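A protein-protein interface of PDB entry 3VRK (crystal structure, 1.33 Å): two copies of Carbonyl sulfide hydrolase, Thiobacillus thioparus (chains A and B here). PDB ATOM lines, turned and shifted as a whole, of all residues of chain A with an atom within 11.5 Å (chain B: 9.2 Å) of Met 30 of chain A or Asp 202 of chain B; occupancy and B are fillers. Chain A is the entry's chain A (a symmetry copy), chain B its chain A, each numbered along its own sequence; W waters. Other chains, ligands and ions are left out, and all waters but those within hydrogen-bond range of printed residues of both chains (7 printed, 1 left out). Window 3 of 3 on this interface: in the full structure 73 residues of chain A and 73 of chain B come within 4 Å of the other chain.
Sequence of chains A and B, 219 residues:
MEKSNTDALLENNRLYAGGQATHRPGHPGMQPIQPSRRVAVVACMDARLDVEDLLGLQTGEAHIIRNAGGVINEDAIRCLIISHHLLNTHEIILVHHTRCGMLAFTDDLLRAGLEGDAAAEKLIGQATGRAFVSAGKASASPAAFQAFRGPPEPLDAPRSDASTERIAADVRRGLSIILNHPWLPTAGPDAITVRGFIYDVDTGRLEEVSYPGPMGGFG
The guanidinium group (NH1) of Arg 48 of chain B lies within hydrogen-bond range of the backbone carbonyl oxygen (O) of Gln 31 of chain A, at 3.0 Å. OD2 of Asp 156 of chain B lies within hydrogen-bond range of N of Ile 33 of chain A. A ring nitrogen (ND1) of His 27 of chain A lies within hydrogen-bond range of the side-chain hydroxyl of Tyr 199 of chain B (3.2 Å). The backbone carbonyl oxygen of Val 201 of chain B sits close to a ring nitrogen (NE2) of His 27 of chain A, 3.4 Å away. O of Asp 202 of chain B sits at hydrogen-bond distance from NE2 of His 27 of chain A, at 3.4 Å.
The guanidinium group (NH2) of Arg 48 of chain B is in salt-bridge range of the side-chain carboxylate (OD2) of Asp 46 of chain B (2.9 Å). OD1 of Asp 156 of chain B is in salt-bridge range of NH1 of Arg 48 of chain B (2.8 Å). The side-chain hydroxyl (OG1) of Thr 98 of chain B lies within hydrogen-bond range of the backbone NH (N) of Val 201 of chain B (3.1 Å). OD1 of Asp 200 of chain B lies within hydrogen-bond range of N of Asp 202 of chain B, at 2.9 Å. A ring nitrogen (NE2) of His 27 of chain A sits close to the backbone NH of Gly 29 of chain A, at 3.4 Å. The side-chain amide nitrogen (NE2) of Gln 31 of chain A sits at hydrogen-bond distance from the backbone carbonyl oxygen (O) of Thr 59 of chain A, 2.9 Å away.
CE1 of Tyr 16 of chain B touches C of Gly 26 of chain A (3.5 Å). Tyr 16 of chain B touches His 27 of chain A. Gly 204 of chain B touches His 27 of chain A (N to CE1, 3.7 Å). Tyr 16 of chain B touches Pro 28 of chain A (OH to CD, 3.95 Å). CD of Arg 48 of chain B touches O of Pro 32 of chain A (3.5 Å). Pro 32 of chain A touches Asp 156 of chain B. CG1 of Ile 33 of chain A touches OD2 of Asp 46 of chain B (3.5 Å). Ile 33 of chain A touches Arg 48 of chain B (CB to NH2, 3.5 Å). Arg 99 of chain B touches Ile 33 of chain A. Thr 59 of chain A touches Arg 48 of chain B (CG2 to O, 3.2 Å).
Printed residues of chain B within 4 Å of Gly 26 of chain A: Tyr 16. Printed residues of chain B within 4 Å of His 27 of chain A: Tyr 16, Tyr 199, Val 201, Asp 202 and Gly 204. No residue of chain B comes within 4 Å of Gly 29 of chain A. Met 30 of chain A touches just one residue of chain B: Asp 202. Glu 61 of chain A touches none of the printed residues of chain B. Of the printed residues of chain A, Arg 48 of chain B touches Gln 31, Pro 32, Ile 33 and Thr 59. Of the printed residues of chain A, Asp 156 of chain B touches Pro 32 and Ile 33. No residue of chain A comes within 4 Å of Pro 158 of chain B. Printed residues of chain A within 4 Å of Tyr 199 of chain B: His 27 (3.2 Å). No residue of chain A comes within 4 Å of Asp 200 of chain B. Val 201 of chain B touches just one residue of chain A: His 27 (2.9 Å). Asp 202 of chain B touches two residues of chain A. Gly 204 of chain B touches just one residue of chain A: His 27. The nearest residue of chain B that does not touch Met 30 of chain A is Arg 99 of chain B (4.1 Å). The nearest printed residue of chain B that does not touch Gly 26 of chain A is Tyr 199 of chain B (7.3 Å).
Hydrophobic or aromatic side chains of chain A within 4 Å of the printed part of chain B: His 27, Pro 28, Met 30 and Ile 33. Hydrophobic or aromatic side chains of chain B that line the printed part of chain A: Tyr 16 and Tyr 199.
No position is printed for both chains.
Water W7 lies within hydrogen-bond range of the side-chain carboxylate (OD2) of Asp 156 of chain B (2.6 Å) and the side-chain amide oxygen (OE1) of Gln 34 of chain A (3.0 Å). Water W5 lies within hydrogen-bond range of OH of Tyr 199 of chain B (2.7 Å), O of Arg 48 of chain B (2.7 Å), O of Val 201 of chain B (3.3 Å) and ND1 of His 27 of chain A (3.5 Å). Water W3 bridges the backbone carbonyl oxygen (O) of Ile 33 of chain A (2.7 Å) and the side-chain carboxylate (OD2) of Asp 46 of chain B (3.4 Å). Water W4 lies within hydrogen-bond range of the backbone carbonyl oxygen of Gly 26 of chain A (2.8 Å), the side-chain hydroxyl of Tyr 16 of chain B (2.8 Å) and the side-chain hydroxyl of Thr 59 of chain A (2.8 Å). Water W2 lies within hydrogen-bond range of OD1 of Asp 202 of chain B (2.8 Å), N of Gln 31 of chain A (2.9 Å) and O of Val 201 of chain B (3.3 Å). Water W6 lies within hydrogen-bond range of N of His 27 of chain A and O of Tyr 16 of chain B.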
ATOM      1  N   GLY A  26       8.606 -20.543  31.308  1.00  0.00           N
ATOM      2  CA  GLY A  26       8.643 -19.913  29.992  1.00  0.00           C
ATOM      3  C   GLY A  26       7.273 -19.771  29.341  1.00  0.00           C
ATOM      4  O   GLY A  26       6.269 -20.374  29.731  1.00  0.00           O
ATOM      5  N   HIS A  27       7.204 -18.977  28.285  1.00  0.00           N
ATOM      6  CA  HIS A  27       5.966 -18.779  27.519  1.00  0.00           C
ATOM      7  C   HIS A  27       5.603 -20.059  26.787  1.00  0.00           C
ATOM      8  O   HIS A  27       6.504 -20.625  26.120  1.00  0.00           O
ATOM      9  CB  HIS A  27       6.183 -17.603  26.561  1.00  0.00           C
ATOM     10  CG  HIS A  27       4.992 -17.331  25.711  1.00  0.00           C
ATOM     11  ND1 HIS A  27       3.801 -16.793  26.146  1.00  0.00           N
ATOM     12  CD2 HIS A  27       4.832 -17.557  24.387  1.00  0.00           C
ATOM     13  CE1 HIS A  27       2.955 -16.684  25.119  1.00  0.00           C
ATOM     14  NE2 HIS A  27       3.574 -17.142  24.067  1.00  0.00           N
ATOM     15  N   PRO A  28       4.382 -20.564  26.898  1.00  0.00           N
ATOM     16  CA  PRO A  28       4.011 -21.830  26.256  1.00  0.00           C
ATOM     17  C   PRO A  28       3.627 -21.716  24.789  1.00  0.00           C
ATOM     18  O   PRO A  28       3.261 -22.732  24.181  1.00  0.00           O
ATOM     19  CB  PRO A  28       2.800 -22.276  27.103  1.00  0.00           C
ATOM     20  CG  PRO A  28       2.164 -20.991  27.507  1.00  0.00           C
ATOM     21  CD  PRO A  28       3.323 -20.046  27.764  1.00  0.00           C
ATOM     22  N   GLY A  29       3.703 -20.528  24.177  1.00  0.00           N
ATOM     23  CA  GLY A  29       3.224 -20.425  22.807  1.00  0.00           C
ATOM     24  C   GLY A  29       1.714 -20.218  22.774  1.00  0.00           C
ATOM     25  O   GLY A  29       1.068 -19.975  23.790  1.00  0.00           O
ATOM     26  N   MET A  30       1.119 -20.335  21.584  1.00  0.00           N
ATOM     27  CA  MET A  30      -0.309 -20.086  21.413  1.00  0.00           C
ATOM     28  C   MET A  30      -1.159 -21.176  22.061  1.00  0.00           C
ATOM     29  O   MET A  30      -0.871 -22.362  21.940  1.00  0.00           O
ATOM     30  CB  MET A  30      -0.688 -20.011  19.907  1.00  0.00           C
ATOM     31  CG  MET A  30       0.098 -18.892  19.226  1.00  0.00           C
ATOM     32  SD  MET A  30      -0.375 -18.671  17.500  1.00  0.00           S
ATOM     33  CE  MET A  30      -2.154 -18.814  17.526  1.00  0.00           C
ATOM     34  N   GLN A  31      -2.225 -20.750  22.732  1.00  0.00           N
ATOM     35  CA  GLN A  31      -3.107 -21.644  23.449  1.00  0.00           C
ATOM     36  C   GLN A  31      -4.561 -21.154  23.347  1.00  0.00           C
ATOM     37  O   GLN A  31      -4.830 -19.962  23.176  1.00  0.00           O
ATOM     38  CB  GLN A  31      -2.738 -21.671  24.934  1.00  0.00           C
ATOM     39  CG  GLN A  31      -1.361 -22.272  25.227  1.00  0.00           C
ATOM     40  CD  GLN A  31      -1.037 -22.134  26.732  1.00  0.00           C
ATOM     41  OE1 GLN A  31      -1.131 -21.059  27.346  1.00  0.00           O
ATOM     42  NE2 GLN A  31      -0.629 -23.228  27.335  1.00  0.00           N
ATOM     43  N   PRO A  32      -5.479 -22.087  23.520  1.00  0.00           N
ATOM     44  CA  PRO A  32      -6.900 -21.710  23.585  1.00  0.00           C
ATOM     45  C   PRO A  32      -7.307 -21.171  24.947  1.00  0.00           C
ATOM     46  O   PRO A  32      -6.660 -21.394  25.980  1.00  0.00           O
ATOM     47  CB  PRO A  32      -7.571 -23.054  23.300  1.00  0.00           C
ATOM     48  CG  PRO A  32      -6.648 -24.038  23.983  1.00  0.00           C
ATOM     49  CD  PRO A  32      -5.256 -23.560  23.620  1.00  0.00           C
ATOM     50  N   ILE A  33      -8.409 -20.399  24.957  1.00  0.00           N
ATOM     51  CA  ILE A  33      -8.834 -19.736  26.184  1.00  0.00           C
ATOM     52  C   ILE A  33      -9.305 -20.714  27.242  1.00  0.00           C
ATOM     53  O   ILE A  33      -9.138 -20.478  28.450  1.00  0.00           O
ATOM     54  CB  ILE A  33      -9.943 -18.679  25.896  1.00  0.00           C
ATOM     55  CG1 ILE A  33     -10.229 -17.870  27.151  1.00  0.00           C
ATOM     56  CG2 ILE A  33     -11.205 -19.310  25.297  1.00  0.00           C
ATOM     57  CD1 ILE A  33     -11.088 -16.627  26.953  1.00  0.00           C
ATOM     58  N   GLN A  34      -9.920 -21.832  26.858  1.00  0.00           N
ATOM     59  CA  GLN A  34     -10.473 -22.749  27.863  1.00  0.00           C
ATOM     60  C   GLN A  34      -9.343 -23.360  28.685  1.00  0.00           C
ATOM     61  O   GLN A  34      -8.407 -23.942  28.097  1.00  0.00           O
ATOM     62  CB  GLN A  34     -11.290 -23.840  27.154  1.00  0.00           C
ATOM     63  CG  GLN A  34     -12.574 -23.315  26.529  1.00  0.00           C
ATOM     64  CD  GLN A  34     -12.426 -22.693  25.154  1.00  0.00           C
ATOM     65  OE1 GLN A  34     -11.343 -22.753  24.553  1.00  0.00           O
ATOM     66  NE2 GLN A  34     -13.531 -22.122  24.647  1.00  0.00           N
ATOM     67  N   SER A  36      -7.032 -25.888  30.226  1.00  0.00           N
ATOM     68  CA  SER A  36      -6.982 -27.278  29.715  1.00  0.00           C
ATOM     69  C   SER A  36      -7.263 -28.307  30.817  1.00  0.00           C
ATOM     70  O   SER A  36      -7.674 -29.450  30.552  1.00  0.00           O
ATOM     71  CB  SER A  36      -5.634 -27.557  29.059  1.00  0.00           C
ATOM     72  OG  SER A  36      -4.587 -27.424  30.013  1.00  0.00           O
ATOM     73  N   THR A  59       1.201 -23.090  32.651  1.00  0.00           N
ATOM     74  CA  THR A  59       0.448 -21.989  32.020  1.00  0.00           C
ATOM     75  C   THR A  59      -0.536 -22.557  31.012  1.00  0.00           C
ATOM     76  O   THR A  59      -0.147 -23.393  30.192  1.00  0.00           O
ATOM     77  CB  THR A  59       1.446 -21.033  31.350  1.00  0.00           C
ATOM     78  OG1 THR A  59       2.380 -20.693  32.393  1.00  0.00           O
ATOM     79  CG2 THR A  59       0.764 -19.784  30.812  1.00  0.00           C
ATOM     80  N   GLY A  60      -1.797 -22.132  31.064  1.00  0.00           N
ATOM     81  CA  GLY A  60      -2.836 -22.590  30.169  1.00  0.00           C
ATOM     82  C   GLY A  60      -3.790 -23.599  30.778  1.00  0.00           C
ATOM     83  O   GLY A  60      -4.853 -23.874  30.168  1.00  0.00           O
ATOM     84  N   GLU A  61      -3.450 -24.140  31.966  1.00  0.00           N
ATOM     85  CA  GLU A  61      -4.213 -25.210  32.579  1.00  0.00           C
ATOM     86  C   GLU A  61      -5.361 -24.745  33.475  1.00  0.00           C
ATOM     87  O   GLU A  61      -6.371 -25.487  33.517  1.00  0.00           O
ATOM     88  CB  GLU A  61      -3.328 -26.098  33.477  1.00  0.00           C
ATOM     89  CG  GLU A  61      -2.389 -26.997  32.648  1.00  0.00           C
ATOM     90  CD  GLU A  61      -1.921 -28.170  33.508  1.00  0.00           C
ATOM     91  OE1 GLU A  61      -1.174 -27.952  34.465  1.00  0.00           O
ATOM     92  OE2 GLU A  61      -2.355 -29.319  33.249  1.00  0.00           O
ATOM     93  N   TYR B  16      10.918 -12.962  28.015  1.00  0.00           N
ATOM     94  CA  TYR B  16       9.877 -13.999  28.068  1.00  0.00           C
ATOM     95  C   TYR B  16       9.274 -14.191  26.692  1.00  0.00           C
ATOM     96  O   TYR B  16       9.122 -15.318  26.190  1.00  0.00           O
ATOM     97  CB  TYR B  16       8.819 -13.593  29.053  1.00  0.00           C
ATOM     98  CG  TYR B  16       7.643 -14.505  29.298  1.00  0.00           C
ATOM     99  CD1 TYR B  16       7.778 -15.665  30.065  1.00  0.00           C
ATOM    100  CD2 TYR B  16       6.391 -14.178  28.764  1.00  0.00           C
ATOM    101  CE1 TYR B  16       6.672 -16.497  30.283  1.00  0.00           C
ATOM    102  CE2 TYR B  16       5.297 -14.993  29.000  1.00  0.00           C
ATOM    103  CZ  TYR B  16       5.438 -16.138  29.759  1.00  0.00           C
ATOM    104  OH  TYR B  16       4.321 -16.923  29.970  1.00  0.00           O
ATOM    105  N   ALA B  17       8.923 -13.066  26.054  1.00  0.00           N
ATOM    106  CA  ALA B  17       8.352 -13.113  24.713  1.00  0.00           C
ATOM    107  C   ALA B  17       9.276 -13.773  23.715  1.00  0.00           C
ATOM    108  O   ALA B  17       8.828 -14.452  22.785  1.00  0.00           O
ATOM    109  CB  ALA B  17       8.025 -11.678  24.280  1.00  0.00           C
ATOM    110  N   GLY B  18      10.582 -13.542  23.888  1.00  0.00           N
ATOM    111  CA  GLY B  18      11.605 -14.107  23.028  1.00  0.00           C
ATOM    112  C   GLY B  18      11.985 -15.541  23.365  1.00  0.00           C
ATOM    113  O   GLY B  18      12.844 -16.079  22.656  1.00  0.00           O
ATOM    114  N   ASP B  46      -7.370 -15.392  33.188  1.00  0.00           N
ATOM    115  CA  ASP B  46      -7.162 -16.237  32.039  1.00  0.00           C
ATOM    116  C   ASP B  46      -5.977 -17.184  32.234  1.00  0.00           C
ATOM    117  O   ASP B  46      -4.891 -16.762  32.660  1.00  0.00           O
ATOM    118  CB  ASP B  46      -6.898 -15.324  30.818  1.00  0.00           C
ATOM    119  CG  ASP B  46      -6.861 -16.044  29.493  1.00  0.00           C
ATOM    120  OD1 ASP B  46      -5.891 -16.805  29.262  1.00  0.00           O
ATOM    121  OD2 ASP B  46      -7.773 -15.832  28.659  1.00  0.00           O
ATOM    122  N   ARG B  48      -3.929 -18.551  30.419  1.00  0.00           N
ATOM    123  CA  ARG B  48      -2.719 -18.348  29.606  1.00  0.00           C
ATOM    124  C   ARG B  48      -1.802 -17.303  30.208  1.00  0.00           C
ATOM    125  O   ARG B  48      -0.681 -17.112  29.708  1.00  0.00           O
ATOM    126  CB  ARG B  48      -3.132 -17.970  28.174  1.00  0.00           C
ATOM    127  CG  ARG B  48      -3.992 -19.048  27.507  1.00  0.00           C
ATOM    128  CD  ARG B  48      -4.548 -18.586  26.167  1.00  0.00           C
ATOM    129  NE  ARG B  48      -5.628 -17.608  26.420  1.00  0.00           N
ATOM    130  CZ  ARG B  48      -6.439 -17.158  25.492  1.00  0.00           C
ATOM    131  NH1 ARG B  48      -6.342 -17.564  24.227  1.00  0.00           N
ATOM    132  NH2 ARG B  48      -7.386 -16.282  25.851  1.00  0.00           N
ATOM    133  N   LEU B  49      -2.252 -16.610  31.258  1.00  0.00           N
ATOM    134  CA  LEU B  49      -1.392 -15.649  31.940  1.00  0.00           C
ATOM    135  C   LEU B  49      -0.838 -16.329  33.193  1.00  0.00           C
ATOM    136  O   LEU B  49      -1.604 -16.771  34.062  1.00  0.00           O
ATOM    137  CB  LEU B  49      -2.131 -14.406  32.394  1.00  0.00           C
ATOM    138  CG  LEU B  49      -2.298 -13.306  31.343  1.00  0.00           C
ATOM    139  CD1 LEU B  49      -3.163 -13.832  30.230  1.00  0.00           C
ATOM    140  CD2 LEU B  49      -2.883 -12.080  32.007  1.00  0.00           C
ATOM    141  N   HIS B  97      -5.280  -8.341  28.571  1.00  0.00           N
ATOM    142  CA  HIS B  97      -4.573  -9.197  27.576  1.00  0.00           C
ATOM    143  C   HIS B  97      -5.455  -9.434  26.360  1.00  0.00           C
ATOM    144  O   HIS B  97      -6.682  -9.270  26.395  1.00  0.00           O
ATOM    145  CB  HIS B  97      -4.113 -10.536  28.211  1.00  0.00           C
ATOM    146  CG  HIS B  97      -5.329 -11.384  28.433  1.00  0.00           C
ATOM    147  ND1 HIS B  97      -5.758 -12.361  27.561  1.00  0.00           N
ATOM    148  CD2 HIS B  97      -6.278 -11.330  29.421  1.00  0.00           C
ATOM    149  CE1 HIS B  97      -6.889 -12.880  28.028  1.00  0.00           C
ATOM    150  NE2 HIS B  97      -7.238 -12.287  29.157  1.00  0.00           N
ATOM    151  N   THR B  98      -4.834  -9.848  25.283  1.00  0.00           N
ATOM    152  CA  THR B  98      -5.535 -10.149  24.050  1.00  0.00           C
ATOM    153  C   THR B  98      -6.285 -11.474  24.131  1.00  0.00           C
ATOM    154  O   THR B  98      -5.930 -12.350  24.907  1.00  0.00           O
ATOM    155  CB  THR B  98      -4.552 -10.218  22.861  1.00  0.00           C
ATOM    156  OG1 THR B  98      -3.559 -11.218  23.110  1.00  0.00           O
ATOM    157  CG2 THR B  98      -3.837  -8.891  22.674  1.00  0.00           C
ATOM    158  N   ARG B  99      -7.305 -11.602  23.276  1.00  0.00           N
ATOM    159  CA  ARG B  99      -8.141 -12.799  23.195  1.00  0.00           C
ATOM    160  C   ARG B  99      -8.885 -13.015  24.528  1.00  0.00           C
ATOM    161  O   ARG B  99      -9.222 -14.146  24.868  1.00  0.00           O
ATOM    162  CB  ARG B  99      -7.347 -14.041  22.757  1.00  0.00           C
ATOM    163  CG  ARG B  99      -6.394 -13.809  21.582  1.00  0.00           C
ATOM    164  CD  ARG B  99      -5.719 -15.112  21.134  1.00  0.00           C
ATOM    165  NE  ARG B  99      -6.634 -15.856  20.304  1.00  0.00           N
ATOM    166  CZ  ARG B  99      -6.384 -16.349  19.092  1.00  0.00           C
ATOM    167  NH1 ARG B  99      -5.200 -16.228  18.537  1.00  0.00           N
ATOM    168  NH2 ARG B  99      -7.311 -16.987  18.420  1.00  0.00           N
ATOM    169  N   ASP B 156     -12.405 -15.981  21.979  1.00  0.00           N
ATOM    170  CA  ASP B 156     -11.015 -16.314  21.656  1.00  0.00           C
ATOM    171  C   ASP B 156     -10.653 -15.927  20.221  1.00  0.00           C
ATOM    172  O   ASP B 156      -9.823 -16.603  19.604  1.00  0.00           O
ATOM    173  CB  ASP B 156     -10.755 -17.806  21.897  1.00  0.00           C
ATOM    174  CG  ASP B 156      -9.332 -18.138  22.251  1.00  0.00           C
ATOM    175  OD1 ASP B 156      -8.523 -17.203  22.508  1.00  0.00           O
ATOM    176  OD2 ASP B 156      -8.954 -19.334  22.311  1.00  0.00           O
ATOM    177  N   ALA B 157     -11.213 -14.881  19.667  1.00  0.00           N
ATOM    178  CA  ALA B 157     -10.844 -14.402  18.347  1.00  0.00           C
ATOM    179  C   ALA B 157      -9.413 -13.852  18.333  1.00  0.00           C
ATOM    180  O   ALA B 157      -8.968 -13.321  19.390  1.00  0.00           O
ATOM    181  CB  ALA B 157     -11.803 -13.307  17.874  1.00  0.00           C
ATOM    182  N   PRO B 158      -8.730 -13.966  17.193  1.00  0.00           N
ATOM    183  CA  PRO B 158      -7.398 -13.377  17.055  1.00  0.00           C
ATOM    184  C   PRO B 158      -7.410 -11.849  17.198  1.00  0.00           C
ATOM    185  O   PRO B 158      -8.471 -11.216  17.089  1.00  0.00           O
ATOM    186  CB  PRO B 158      -6.980 -13.703  15.613  1.00  0.00           C
ATOM    187  CG  PRO B 158      -8.117 -14.356  14.923  1.00  0.00           C
ATOM    188  CD  PRO B 158      -9.161 -14.659  15.956  1.00  0.00           C
ATOM    189  N   ARG B 159      -6.292 -11.207  17.465  1.00  0.00           N
ATOM    190  CA  ARG B 159      -6.170  -9.789  17.657  1.00  0.00           C
ATOM    191  C   ARG B 159      -6.690  -8.968  16.490  1.00  0.00           C
ATOM    192  O   ARG B 159      -6.558  -9.411  15.351  1.00  0.00           O
ATOM    193  CB  ARG B 159      -4.696  -9.296  17.676  1.00  0.00           C
ATOM    194  CG  ARG B 159      -3.919  -9.817  18.847  1.00  0.00           C
ATOM    195  CD  ARG B 159      -2.630  -8.982  18.926  1.00  0.00           C
ATOM    196  NE  ARG B 159      -3.034  -7.608  19.289  1.00  0.00           N
ATOM    197  CZ  ARG B 159      -2.282  -6.831  20.045  1.00  0.00           C
ATOM    198  NH1 ARG B 159      -1.120  -7.305  20.503  1.00  0.00           N
ATOM    199  NH2 ARG B 159      -2.664  -5.597  20.363  1.00  0.00           N
ATOM    200  N   SER B 160      -7.147  -7.782  16.826  1.00  0.00           N
ATOM    201  CA  SER B 160      -7.388  -6.795  15.775  1.00  0.00           C
ATOM    202  C   SER B 160      -7.200  -5.401  16.357  1.00  0.00           C
ATOM    203  O   SER B 160      -7.196  -5.242  17.558  1.00  0.00           O
ATOM    204  CB  SER B 160      -8.804  -6.982  15.242  1.00  0.00           C
ATOM    205  OG  SER B 160      -9.766  -6.646  16.255  1.00  0.00           O
ATOM    206  N   TYR B 199      -1.182  -7.577  27.538  1.00  0.00           N
ATOM    207  CA  TYR B 199      -0.332  -8.728  27.301  1.00  0.00           C
ATOM    208  C   TYR B 199      -0.831  -9.466  26.063  1.00  0.00           C
ATOM    209  O   TYR B 199      -2.012  -9.864  26.038  1.00  0.00           O
ATOM    210  CB  TYR B 199      -0.373  -9.626  28.553  1.00  0.00           C
ATOM    211  CG  TYR B 199       0.326 -10.958  28.340  1.00  0.00           C
ATOM    212  CD1 TYR B 199       1.704 -11.052  28.186  1.00  0.00           C
ATOM    213  CD2 TYR B 199      -0.426 -12.127  28.301  1.00  0.00           C
ATOM    214  CE1 TYR B 199       2.299 -12.301  28.003  1.00  0.00           C
ATOM    215  CE2 TYR B 199       0.149 -13.377  28.101  1.00  0.00           C
ATOM    216  CZ  TYR B 199       1.527 -13.441  27.956  1.00  0.00           C
ATOM    217  OH  TYR B 199       2.133 -14.638  27.735  1.00  0.00           O
ATOM    218  N   ASP B 200       0.029  -9.660  25.067  1.00  0.00           N
ATOM    219  CA  ASP B 200      -0.324 -10.467  23.896  1.00  0.00           C
ATOM    220  C   ASP B 200      -0.110 -11.935  24.234  1.00  0.00           C
ATOM    221  O   ASP B 200       1.028 -12.375  24.387  1.00  0.00           O
ATOM    222  CB  ASP B 200       0.486  -9.976  22.710  1.00  0.00           C
ATOM    223  CG  ASP B 200       0.119 -10.628  21.412  1.00  0.00           C
ATOM    224  OD1 ASP B 200      -0.149 -11.863  21.417  1.00  0.00           O
ATOM    225  OD2 ASP B 200       0.138  -9.898  20.388  1.00  0.00           O
ATOM    226  N   VAL B 201      -1.197 -12.709  24.342  1.00  0.00           N
ATOM    227  CA  VAL B 201      -1.016 -14.100  24.791  1.00  0.00           C
ATOM    228  C   VAL B 201      -0.250 -14.947  23.778  1.00  0.00           C
ATOM    229  O   VAL B 201       0.356 -15.978  24.128  1.00  0.00           O
ATOM    230  CB  VAL B 201      -2.370 -14.790  25.105  1.00  0.00           C
ATOM    231  CG1 VAL B 201      -3.058 -14.157  26.323  1.00  0.00           C
ATOM    232  CG2 VAL B 201      -3.326 -14.749  23.904  1.00  0.00           C
ATOM    233  N   ASP B 202      -0.308 -14.553  22.511  1.00  0.00           N
ATOM    234  CA  ASP B 202       0.328 -15.366  21.457  1.00  0.00           C
ATOM    235  C   ASP B 202       1.815 -15.065  21.325  1.00  0.00           C
ATOM    236  O   ASP B 202       2.602 -15.973  21.079  1.00  0.00           O
ATOM    237  CB  ASP B 202      -0.411 -15.104  20.134  1.00  0.00           C
ATOM    238  CG  ASP B 202      -1.822 -15.668  20.164  1.00  0.00           C
ATOM    239  OD1 ASP B 202      -2.108 -16.579  20.973  1.00  0.00           O
ATOM    240  OD2 ASP B 202      -2.661 -15.175  19.391  1.00  0.00           O
ATOM    241  N   THR B 203       2.238 -13.807  21.473  1.00  0.00           N
ATOM    242  CA  THR B 203       3.636 -13.440  21.344  1.00  0.00           C
ATOM    243  C   THR B 203       4.335 -13.446  22.705  1.00  0.00           C
ATOM    244  O   THR B 203       5.546 -13.542  22.745  1.00  0.00           O
ATOM    245  CB  THR B 203       3.864 -12.037  20.716  1.00  0.00           C
ATOM    246  OG1 THR B 203       3.310 -11.076  21.629  1.00  0.00           O
ATOM    247  CG2 THR B 203       3.197 -11.953  19.368  1.00  0.00           C
ATOM    248  N   GLY B 204       3.621 -13.301  23.798  1.00  0.00           N
ATOM    249  CA  GLY B 204       4.181 -13.180  25.125  1.00  0.00           C
ATOM    250  C   GLY B 204       4.604 -11.778  25.463  1.00  0.00           C
ATOM    251  O   GLY B 204       5.165 -11.610  26.582  1.00  0.00           O
ATOM    252  N   ARG B 205       4.370 -10.778  24.614  1.00  0.00           N
ATOM    253  CA  ARG B 205       4.878  -9.431  24.854  1.00  0.00           C
ATOM    254  C   ARG B 205       3.801  -8.455  25.337  1.00  0.00           C
ATOM    255  O   ARG B 205       2.674  -8.441  24.833  1.00  0.00           O
ATOM    256  CB  ARG B 205       5.481  -8.913  23.531  1.00  0.00           C
ATOM    257  CG  ARG B 205       6.340  -7.676  23.718  1.00  0.00           C
ATOM    258  CD  ARG B 205       7.691  -8.022  24.345  1.00  0.00           C
ATOM    259  NE  ARG B 205       8.547  -6.820  24.513  1.00  0.00           N
ATOM    260  CZ  ARG B 205       9.299  -6.221  23.593  1.00  0.00           C
ATOM    261  NH1 ARG B 205      10.018  -5.141  23.894  1.00  0.00           N
ATOM    262  NH2 ARG B 205       9.326  -6.717  22.345  1.00  0.00           N
ATOM    263  N   LEU B 206       4.200  -7.645  26.315  1.00  0.00           N
ATOM    264  CA  LEU B 206       3.361  -6.531  26.779  1.00  0.00           C
ATOM    265  C   LEU B 206       3.470  -5.299  25.888  1.00  0.00           C
ATOM    266  O   LEU B 206       4.536  -5.050  25.289  1.00  0.00           O
ATOM    267  CB  LEU B 206       3.825  -6.118  28.172  1.00  0.00           C
ATOM    268  CG  LEU B 206       3.571  -7.133  29.279  1.00  0.00           C
ATOM    269  CD1 LEU B 206       4.461  -6.811  30.476  1.00  0.00           C
ATOM    270  CD2 LEU B 206       2.117  -7.113  29.714  1.00  0.00           C
HETATM  271  O   HOH W   1      -4.293 -18.296  20.998  1.00  0.00           O
HETATM  272  O   HOH W   2      -2.145 -17.952  23.424  1.00  0.00           O
HETATM  273  O   HOH W   3      -8.722 -18.616  30.345  1.00  0.00           O
HETATM  274  O   HOH W   4       4.612 -19.155  31.579  1.00  0.00           O
HETATM  275  O   HOH W   5       0.517 -16.716  27.300  1.00  0.00           O
HETATM  276  O   HOH W   6       9.635 -17.694  27.666  1.00  0.00           O
HETATM  277  O   HOH W   7     -10.555 -21.385  21.994  1.00  0.00           O
